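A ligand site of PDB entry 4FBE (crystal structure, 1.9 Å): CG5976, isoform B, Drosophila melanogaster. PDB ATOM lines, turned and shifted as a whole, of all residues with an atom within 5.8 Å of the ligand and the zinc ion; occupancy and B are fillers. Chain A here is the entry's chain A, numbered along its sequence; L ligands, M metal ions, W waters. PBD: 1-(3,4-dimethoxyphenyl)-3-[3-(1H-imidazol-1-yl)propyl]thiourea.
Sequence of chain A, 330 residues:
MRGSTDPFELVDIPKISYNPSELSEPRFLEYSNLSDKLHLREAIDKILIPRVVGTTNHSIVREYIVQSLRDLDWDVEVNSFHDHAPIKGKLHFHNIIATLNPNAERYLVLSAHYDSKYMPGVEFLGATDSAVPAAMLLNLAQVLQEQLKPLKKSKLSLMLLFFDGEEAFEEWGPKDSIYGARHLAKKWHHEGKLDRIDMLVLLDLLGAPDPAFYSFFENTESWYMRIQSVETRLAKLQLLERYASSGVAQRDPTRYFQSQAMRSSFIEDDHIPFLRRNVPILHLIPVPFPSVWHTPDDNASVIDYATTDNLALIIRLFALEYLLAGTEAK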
ATOM      1  N   HIS A 113     -11.853  -2.225 -21.139  1.00  0.00           N
ATOM      2  CA  HIS A 113     -10.587  -2.257 -21.885  1.00  0.00           C
ATOM      3  C   HIS A 113      -9.776  -3.495 -21.487  1.00  0.00           C
ATOM      4  O   HIS A 113      -9.746  -3.877 -20.320  1.00  0.00           O
ATOM      5  CB  HIS A 113      -9.780  -0.970 -21.729  1.00  0.00           C
ATOM      6  CG  HIS A 113      -9.040  -0.888 -20.433  1.00  0.00           C
ATOM      7  ND1 HIS A 113      -7.776  -1.432 -20.271  1.00  0.00           N
ATOM      8  CD2 HIS A 113      -9.387  -0.366 -19.233  1.00  0.00           C
ATOM      9  CE1 HIS A 113      -7.389  -1.243 -19.018  1.00  0.00           C
ATOM     10  NE2 HIS A 113      -8.334  -0.584 -18.381  1.00  0.00           N
ATOM     11  N   LYS A 117      -1.707  -1.491 -18.336  1.00  0.00           N
ATOM     12  CA  LYS A 117      -0.831  -0.317 -18.336  1.00  0.00           C
ATOM     13  C   LYS A 117       0.638  -0.731 -18.400  1.00  0.00           C
ATOM     14  O   LYS A 117       1.072  -1.626 -17.697  1.00  0.00           O
ATOM     15  CB  LYS A 117      -1.051   0.534 -17.082  1.00  0.00           C
ATOM     16  CG  LYS A 117      -0.279   1.892 -17.057  1.00  0.00           C
ATOM     17  CD  LYS A 117      -0.909   2.876 -16.049  1.00  0.00           C
ATOM     18  CE  LYS A 117      -0.110   4.192 -15.877  1.00  0.00           C
ATOM     19  NZ  LYS A 117       0.146   4.879 -17.148  1.00  0.00           N
ATOM     20  N   PHE A 124       2.540  -5.303 -13.994  1.00  0.00           N
ATOM     21  CA  PHE A 124       1.251  -4.775 -13.600  1.00  0.00           C
ATOM     22  C   PHE A 124       0.160  -5.647 -14.212  1.00  0.00           C
ATOM     23  O   PHE A 124       0.128  -5.833 -15.414  1.00  0.00           O
ATOM     24  CB  PHE A 124       1.108  -3.328 -14.100  1.00  0.00           C
ATOM     25  CG  PHE A 124      -0.183  -2.685 -13.715  1.00  0.00           C
ATOM     26  CD1 PHE A 124      -0.464  -2.443 -12.388  1.00  0.00           C
ATOM     27  CD2 PHE A 124      -1.116  -2.338 -14.667  1.00  0.00           C
ATOM     28  CE1 PHE A 124      -1.670  -1.857 -12.011  1.00  0.00           C
ATOM     29  CE2 PHE A 124      -2.332  -1.743 -14.286  1.00  0.00           C
ATOM     30  CZ  PHE A 124      -2.598  -1.508 -12.977  1.00  0.00           C
ATOM     31  N   ASP A 129      -8.521  -3.263 -13.310  1.00  0.00           N
ATOM     32  CA  ASP A 129      -8.247  -2.298 -14.357  1.00  0.00           C
ATOM     33  C   ASP A 129      -7.574  -2.913 -15.602  1.00  0.00           C
ATOM     34  O   ASP A 129      -6.391  -2.671 -15.850  1.00  0.00           O
ATOM     35  CB  ASP A 129      -7.307  -1.244 -13.749  1.00  0.00           C
ATOM     36  CG  ASP A 129      -7.068  -0.043 -14.649  1.00  0.00           C
ATOM     37  OD1 ASP A 129      -7.728   0.076 -15.719  1.00  0.00           O
ATOM     38  OD2 ASP A 129      -6.195   0.783 -14.297  1.00  0.00           O
ATOM     39  N   GLU A 166      -6.380   1.557 -23.743  1.00  0.00           N
ATOM     40  CA  GLU A 166      -7.008   2.557 -22.895  1.00  0.00           C
ATOM     41  C   GLU A 166      -5.945   3.327 -22.137  1.00  0.00           C
ATOM     42  O   GLU A 166      -6.082   4.538 -21.955  1.00  0.00           O
ATOM     43  CB  GLU A 166      -8.037   1.941 -21.978  1.00  0.00           C
ATOM     44  CG  GLU A 166      -8.846   2.930 -21.112  1.00  0.00           C
ATOM     45  CD  GLU A 166      -8.193   3.270 -19.767  1.00  0.00           C
ATOM     46  OE1 GLU A 166      -7.051   2.827 -19.498  1.00  0.00           O
ATOM     47  OE2 GLU A 166      -8.864   3.957 -18.972  1.00  0.00           O
ATOM     48  N   GLU A 167      -4.873   2.632 -21.745  1.00  0.00           N
ATOM     49  CA  GLU A 167      -3.880   3.179 -20.837  1.00  0.00           C
ATOM     50  C   GLU A 167      -2.818   3.950 -21.562  1.00  0.00           C
ATOM     51  O   GLU A 167      -2.507   3.685 -22.730  1.00  0.00           O
ATOM     52  CB  GLU A 167      -3.205   2.062 -20.023  1.00  0.00           C
ATOM     53  CG  GLU A 167      -4.152   1.258 -19.219  1.00  0.00           C
ATOM     54  CD  GLU A 167      -4.514   1.906 -17.876  1.00  0.00           C
ATOM     55  OE1 GLU A 167      -4.282   3.119 -17.652  1.00  0.00           O
ATOM     56  OE2 GLU A 167      -5.039   1.187 -17.058  1.00  0.00           O
ATOM     57  N   TRP A 172      -0.705  10.233 -18.964  1.00  0.00           N
ATOM     58  CA  TRP A 172      -2.092  10.281 -19.418  1.00  0.00           C
ATOM     59  C   TRP A 172      -2.454  11.666 -19.932  1.00  0.00           C
ATOM     60  O   TRP A 172      -2.494  12.628 -19.168  1.00  0.00           O
ATOM     61  CB  TRP A 172      -3.045   9.900 -18.288  1.00  0.00           C
ATOM     62  CG  TRP A 172      -4.483   9.908 -18.708  1.00  0.00           C
ATOM     63  CD1 TRP A 172      -5.308  10.995 -18.812  1.00  0.00           C
ATOM     64  CD2 TRP A 172      -5.274   8.768 -19.056  1.00  0.00           C
ATOM     65  NE1 TRP A 172      -6.555  10.603 -19.237  1.00  0.00           N
ATOM     66  CE2 TRP A 172      -6.566   9.239 -19.381  1.00  0.00           C
ATOM     67  CE3 TRP A 172      -5.015   7.392 -19.150  1.00  0.00           C
ATOM     68  CZ2 TRP A 172      -7.603   8.382 -19.772  1.00  0.00           C
ATOM     69  CZ3 TRP A 172      -6.049   6.548 -19.538  1.00  0.00           C
ATOM     70  CH2 TRP A 172      -7.318   7.046 -19.841  1.00  0.00           C
ATOM     71  N   ASP A 204     -15.284  -0.167 -15.527  1.00  0.00           N
ATOM     72  CA  ASP A 204     -13.880   0.056 -15.218  1.00  0.00           C
ATOM     73  C   ASP A 204     -13.646   0.083 -13.696  1.00  0.00           C
ATOM     74  O   ASP A 204     -14.515   0.485 -12.910  1.00  0.00           O
ATOM     75  CB  ASP A 204     -13.437   1.371 -15.846  1.00  0.00           C
ATOM     76  CG  ASP A 204     -11.940   1.439 -16.070  1.00  0.00           C
ATOM     77  OD1 ASP A 204     -11.251   0.469 -15.722  1.00  0.00           O
ATOM     78  OD2 ASP A 204     -11.466   2.456 -16.614  1.00  0.00           O
ATOM     79  N   LEU A 205     -12.462  -0.362 -13.307  1.00  0.00           N
ATOM     80  CA  LEU A 205     -12.039  -0.402 -11.919  1.00  0.00           C
ATOM     81  C   LEU A 205     -13.008  -1.181 -11.012  1.00  0.00           C
ATOM     82  O   LEU A 205     -13.397  -0.705  -9.946  1.00  0.00           O
ATOM     83  CB  LEU A 205     -11.815   1.028 -11.405  1.00  0.00           C
ATOM     84  CG  LEU A 205     -10.891   1.853 -12.303  1.00  0.00           C
ATOM     85  CD1 LEU A 205     -10.541   3.162 -11.670  1.00  0.00           C
ATOM     86  CD2 LEU A 205      -9.611   1.090 -12.678  1.00  0.00           C
ATOM     87  N   PHE A 266     -15.729  14.977 -14.861  1.00  0.00           N
ATOM     88  CA  PHE A 266     -14.879  14.883 -16.061  1.00  0.00           C
ATOM     89  C   PHE A 266     -13.833  13.772 -15.993  1.00  0.00           C
ATOM     90  O   PHE A 266     -12.684  13.957 -16.404  1.00  0.00           O
ATOM     91  CB  PHE A 266     -14.176  16.225 -16.358  1.00  0.00           C
ATOM     92  CG  PHE A 266     -15.130  17.370 -16.599  1.00  0.00           C
ATOM     93  CD1 PHE A 266     -16.000  17.352 -17.687  1.00  0.00           C
ATOM     94  CD2 PHE A 266     -15.146  18.469 -15.744  1.00  0.00           C
ATOM     95  CE1 PHE A 266     -16.871  18.409 -17.926  1.00  0.00           C
ATOM     96  CE2 PHE A 266     -16.019  19.532 -15.975  1.00  0.00           C
ATOM     97  CZ  PHE A 266     -16.884  19.498 -17.064  1.00  0.00           C
ATOM     98  N   ILE A 267     -14.242  12.605 -15.516  1.00  0.00           N
ATOM     99  CA  ILE A 267     -13.370  11.447 -15.478  1.00  0.00           C
ATOM    100  C   ILE A 267     -13.145  11.007 -16.918  1.00  0.00           C
ATOM    101  O   ILE A 267     -14.108  10.855 -17.699  1.00  0.00           O
ATOM    102  CB  ILE A 267     -13.972  10.320 -14.600  1.00  0.00           C
ATOM    103  CG1 ILE A 267     -13.987  10.769 -13.135  1.00  0.00           C
ATOM    104  CG2 ILE A 267     -13.175   9.049 -14.727  1.00  0.00           C
ATOM    105  CD1 ILE A 267     -14.730   9.817 -12.180  1.00  0.00           C
ATOM    106  N   GLU A 268     -11.894  10.868 -17.302  1.00  0.00           N
ATOM    107  CA  GLU A 268     -11.537  10.498 -18.674  1.00  0.00           C
ATOM    108  C   GLU A 268     -11.355   8.975 -18.759  1.00  0.00           C
ATOM    109  O   GLU A 268     -10.785   8.353 -17.873  1.00  0.00           O
ATOM    110  CB  GLU A 268     -10.279  11.236 -19.097  1.00  0.00           C
ATOM    111  CG  GLU A 268     -10.427  12.766 -18.948  1.00  0.00           C
ATOM    112  CD  GLU A 268      -9.305  13.565 -19.573  1.00  0.00           C
ATOM    113  OE1 GLU A 268      -8.292  12.991 -20.051  1.00  0.00           O
ATOM    114  OE2 GLU A 268      -9.471  14.805 -19.603  1.00  0.00           O
ATOM    115  N   ASP A 269     -11.864   8.390 -19.830  1.00  0.00           N
ATOM    116  CA  ASP A 269     -11.846   6.944 -20.034  1.00  0.00           C
ATOM    117  C   ASP A 269     -12.288   6.665 -21.479  1.00  0.00           C
ATOM    118  O   ASP A 269     -12.427   7.590 -22.272  1.00  0.00           O
ATOM    119  CB  ASP A 269     -12.774   6.277 -19.016  1.00  0.00           C
ATOM    120  CG  ASP A 269     -12.411   4.858 -18.702  1.00  0.00           C
ATOM    121  OD1 ASP A 269     -11.560   4.246 -19.374  1.00  0.00           O
ATOM    122  OD2 ASP A 269     -13.026   4.325 -17.783  1.00  0.00           O
ATOM    123  N   ILE A 285     -17.935   3.011 -12.979  1.00  0.00           N
ATOM    124  CA  ILE A 285     -16.614   3.168 -12.435  1.00  0.00           C
ATOM    125  C   ILE A 285     -16.775   3.786 -11.052  1.00  0.00           C
ATOM    126  O   ILE A 285     -17.466   4.782 -10.921  1.00  0.00           O
ATOM    127  CB  ILE A 285     -15.727   4.060 -13.324  1.00  0.00           C
ATOM    128  CG1 ILE A 285     -14.301   4.057 -12.785  1.00  0.00           C
ATOM    129  CG2 ILE A 285     -16.267   5.540 -13.398  1.00  0.00           C
ATOM    130  CD1 ILE A 285     -13.339   4.706 -13.735  1.00  0.00           C
ATOM    131  N   PRO A 286     -16.119   3.190 -10.022  1.00  0.00           N
ATOM    132  CA  PRO A 286     -16.339   3.708  -8.664  1.00  0.00           C
ATOM    133  C   PRO A 286     -15.605   5.022  -8.389  1.00  0.00           C
ATOM    134  O   PRO A 286     -14.595   5.321  -9.028  1.00  0.00           O
ATOM    135  CB  PRO A 286     -15.799   2.590  -7.770  1.00  0.00           C
ATOM    136  CG  PRO A 286     -15.026   1.638  -8.656  1.00  0.00           C
ATOM    137  CD  PRO A 286     -15.084   2.152 -10.059  1.00  0.00           C
ATOM    138  N   VAL A 287     -16.156   5.812  -7.464  1.00  0.00           N
ATOM    139  CA  VAL A 287     -15.548   7.028  -6.961  1.00  0.00           C
ATOM    140  C   VAL A 287     -15.698   6.995  -5.440  1.00  0.00           C
ATOM    141  O   VAL A 287     -16.822   7.002  -4.954  1.00  0.00           O
ATOM    142  CB  VAL A 287     -16.251   8.287  -7.496  1.00  0.00           C
ATOM    143  CG1 VAL A 287     -15.630   9.545  -6.936  1.00  0.00           C
ATOM    144  CG2 VAL A 287     -16.233   8.324  -9.053  1.00  0.00           C
ATOM    145  N   PRO A 288     -14.577   6.932  -4.679  1.00  0.00           N
ATOM    146  CA  PRO A 288     -13.211   6.895  -5.170  1.00  0.00           C
ATOM    147  C   PRO A 288     -12.829   5.620  -5.929  1.00  0.00           C
ATOM    148  O   PRO A 288     -13.451   4.565  -5.753  1.00  0.00           O
ATOM    149  CB  PRO A 288     -12.360   7.044  -3.893  1.00  0.00           C
ATOM    150  CG  PRO A 288     -13.239   6.493  -2.814  1.00  0.00           C
ATOM    151  CD  PRO A 288     -14.626   6.876  -3.201  1.00  0.00           C
ATOM    152  N   PHE A 289     -11.809   5.742  -6.774  1.00  0.00           N
ATOM    153  CA  PHE A 289     -11.167   4.610  -7.437  1.00  0.00           C
ATOM    154  C   PHE A 289     -10.570   3.765  -6.334  1.00  0.00           C
ATOM    155  O   PHE A 289     -10.240   4.278  -5.276  1.00  0.00           O
ATOM    156  CB  PHE A 289      -9.982   5.067  -8.289  1.00  0.00           C
ATOM    157  CG  PHE A 289     -10.351   5.790  -9.555  1.00  0.00           C
ATOM    158  CD1 PHE A 289     -11.650   6.211  -9.820  1.00  0.00           C
ATOM    159  CD2 PHE A 289      -9.366   6.088 -10.471  1.00  0.00           C
ATOM    160  CE1 PHE A 289     -11.952   6.898 -10.975  1.00  0.00           C
ATOM    161  CE2 PHE A 289      -9.661   6.771 -11.647  1.00  0.00           C
ATOM    162  CZ  PHE A 289     -10.946   7.172 -11.907  1.00  0.00           C
ATOM    163  N   TRP A 293      -5.292   1.510  -7.205  1.00  0.00           N
ATOM    164  CA  TRP A 293      -5.235   2.020  -8.588  1.00  0.00           C
ATOM    165  C   TRP A 293      -3.814   2.336  -9.079  1.00  0.00           C
ATOM    166  O   TRP A 293      -3.067   3.059  -8.422  1.00  0.00           O
ATOM    167  CB  TRP A 293      -6.134   3.258  -8.714  1.00  0.00           C
ATOM    168  CG  TRP A 293      -6.283   3.778 -10.111  1.00  0.00           C
ATOM    169  CD1 TRP A 293      -7.021   3.222 -11.125  1.00  0.00           C
ATOM    170  CD2 TRP A 293      -5.685   4.965 -10.648  1.00  0.00           C
ATOM    171  NE1 TRP A 293      -6.901   3.994 -12.267  1.00  0.00           N
ATOM    172  CE2 TRP A 293      -6.093   5.065 -11.990  1.00  0.00           C
ATOM    173  CE3 TRP A 293      -4.841   5.949 -10.116  1.00  0.00           C
ATOM    174  CZ2 TRP A 293      -5.677   6.112 -12.814  1.00  0.00           C
ATOM    175  CZ3 TRP A 293      -4.442   6.984 -10.934  1.00  0.00           C
ATOM    176  CH2 TRP A 293      -4.856   7.059 -12.258  1.00  0.00           C
ATOM    177  N   HIS A 294      -3.446   1.785 -10.243  1.00  0.00           N
ATOM    178  CA  HIS A 294      -2.122   1.976 -10.856  1.00  0.00           C
ATOM    179  C   HIS A 294      -0.923   1.698  -9.939  1.00  0.00           C
ATOM    180  O   HIS A 294       0.117   2.315 -10.070  1.00  0.00           O
ATOM    181  CB  HIS A 294      -2.030   3.376 -11.499  1.00  0.00           C
ATOM    182  CG  HIS A 294      -2.892   3.523 -12.718  1.00  0.00           C
ATOM    183  ND1 HIS A 294      -2.879   4.643 -13.519  1.00  0.00           N
ATOM    184  CD2 HIS A 294      -3.752   2.648 -13.282  1.00  0.00           C
ATOM    185  CE1 HIS A 294      -3.730   4.457 -14.520  1.00  0.00           C
ATOM    186  NE2 HIS A 294      -4.266   3.265 -14.393  1.00  0.00           N
HETATM  187  CAA PBD L   1      -6.899   8.863  -7.773  1.00  0.00           C
HETATM  188  CAB PBD L   1     -11.901  10.331  -9.278  1.00  0.00           C
HETATM  189  SAC PBD L   1      -9.073  12.129 -15.642  1.00  0.00           S
HETATM  190  CAD PBD L   1      -8.704   3.438 -15.470  1.00  0.00           C
HETATM  191  CAE PBD L   1      -7.537  10.398 -11.600  1.00  0.00           C
HETATM  192  CAF PBD L   1      -7.325   9.644 -10.448  1.00  0.00           C
HETATM  193  CAG PBD L   1      -9.149   4.673 -15.712  1.00  0.00           C
HETATM  194  CAH PBD L   1      -7.042   4.596 -16.250  1.00  0.00           C
HETATM  195  CAI PBD L   1      -9.829  10.768 -10.967  1.00  0.00           C
HETATM  196  CAJ PBD L   1      -8.833   7.617 -15.514  1.00  0.00           C
HETATM  197  CAK PBD L   1      -8.661   9.125 -15.700  1.00  0.00           C
HETATM  198  CAL PBD L   1      -8.148   6.801 -16.624  1.00  0.00           C
HETATM  199  NAM PBD L   1      -7.403   3.389 -15.812  1.00  0.00           N
HETATM  200  NAN PBD L   1      -8.729   9.785 -14.372  1.00  0.00           N
HETATM  201  NAO PBD L   1      -8.947  11.661 -12.992  1.00  0.00           N
HETATM  202  OAP PBD L   1      -8.159   8.700  -8.416  1.00  0.00           O
HETATM  203  OAQ PBD L   1     -10.608   9.782  -8.885  1.00  0.00           O
HETATM  204  CAR PBD L   1      -8.882  11.105 -14.222  1.00  0.00           C
HETATM  205  CAS PBD L   1      -8.785  10.958 -11.870  1.00  0.00           C
HETATM  206  CAT PBD L   1      -8.360   9.451  -9.541  1.00  0.00           C
HETATM  207  CAU PBD L   1      -9.614  10.010  -9.798  1.00  0.00           C
HETATM  208  NAV PBD L   1      -8.109   5.367 -16.223  1.00  0.00           N
HETATM  209 ZN    ZN M   1      -5.711   2.138 -15.471  1.00  0.00          ZN
HETATM  210  O   HOH W   1     -10.268   8.490  -6.636  1.00  0.00           O
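Water W1 lies within hydrogen-bond range of an oxygen (OAQ) of the ligand and the backbone NH (N) of Phe 289.
The zinc ion is bound by the side-chain carboxylate (OD2) of Asp 129 (1.9 Å).
The side-chain carboxylate (OE2) of Glu 167 binds the zinc ion (2.0 Å).
A ring nitrogen (NE2) of His 294 is bound to the zinc ion (2.1 Å).
NAM of the ligand binds the zinc ion (2.1 Å).
The zinc ion has four donor atoms within binding distance.
Slightly farther from the zinc ion lies OE1 of Glu 167 (2.8 Å).
The backbone NH of Glu 268 sits close to a sulfur (SAC) of the ligand, at 3.5 Å.
The side-chain carboxylate (OE2) of Glu 166 lies close to a nitrogen (NAV) of the ligand (3.2 Å).
Trp 172 touches the ligand.
Asp 204 touches the ligand.
CD2 of Leu 205 touches CAD of the ligand (3.8 Å).
Phe 289 touches the ligand.
Trp 293 touches the ligand.
Hydrophobic or aromatic side chains that line the ligand: Trp 172, Leu 205, Phe 289, Trp 293 and His 294.
Of the 20 residues printed, 10 come within 4 Å of the ligand.
The side-chain carboxylate of Asp 129 lies within hydrogen-bond range of a ring nitrogen (NE2) of His 113 (2.8 Å).
NE1 of Trp 293 sits close to NE2 of His 294.
OE1 of Glu 268 lies within hydrogen-bond range of NE1 of Trp 172 (3.1 Å).
OD2 of Asp 204 sits close to OD2 of Asp 269.
The side-chain carboxylate (OE2) of Glu 166 lies close to the side-chain carboxylate (OD1) of Asp 269, 2.7 Å away.
Trp 293 touches the zinc ion (NE1 to ZN, 3.9 Å).
Four residues have an atom within 4 Å of the zinc ion: Asp 129, Glu 167, Trp 293 and His 294.
The nearest printed residue that does not touch the zinc ion is Glu 166 (4.3 Å).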
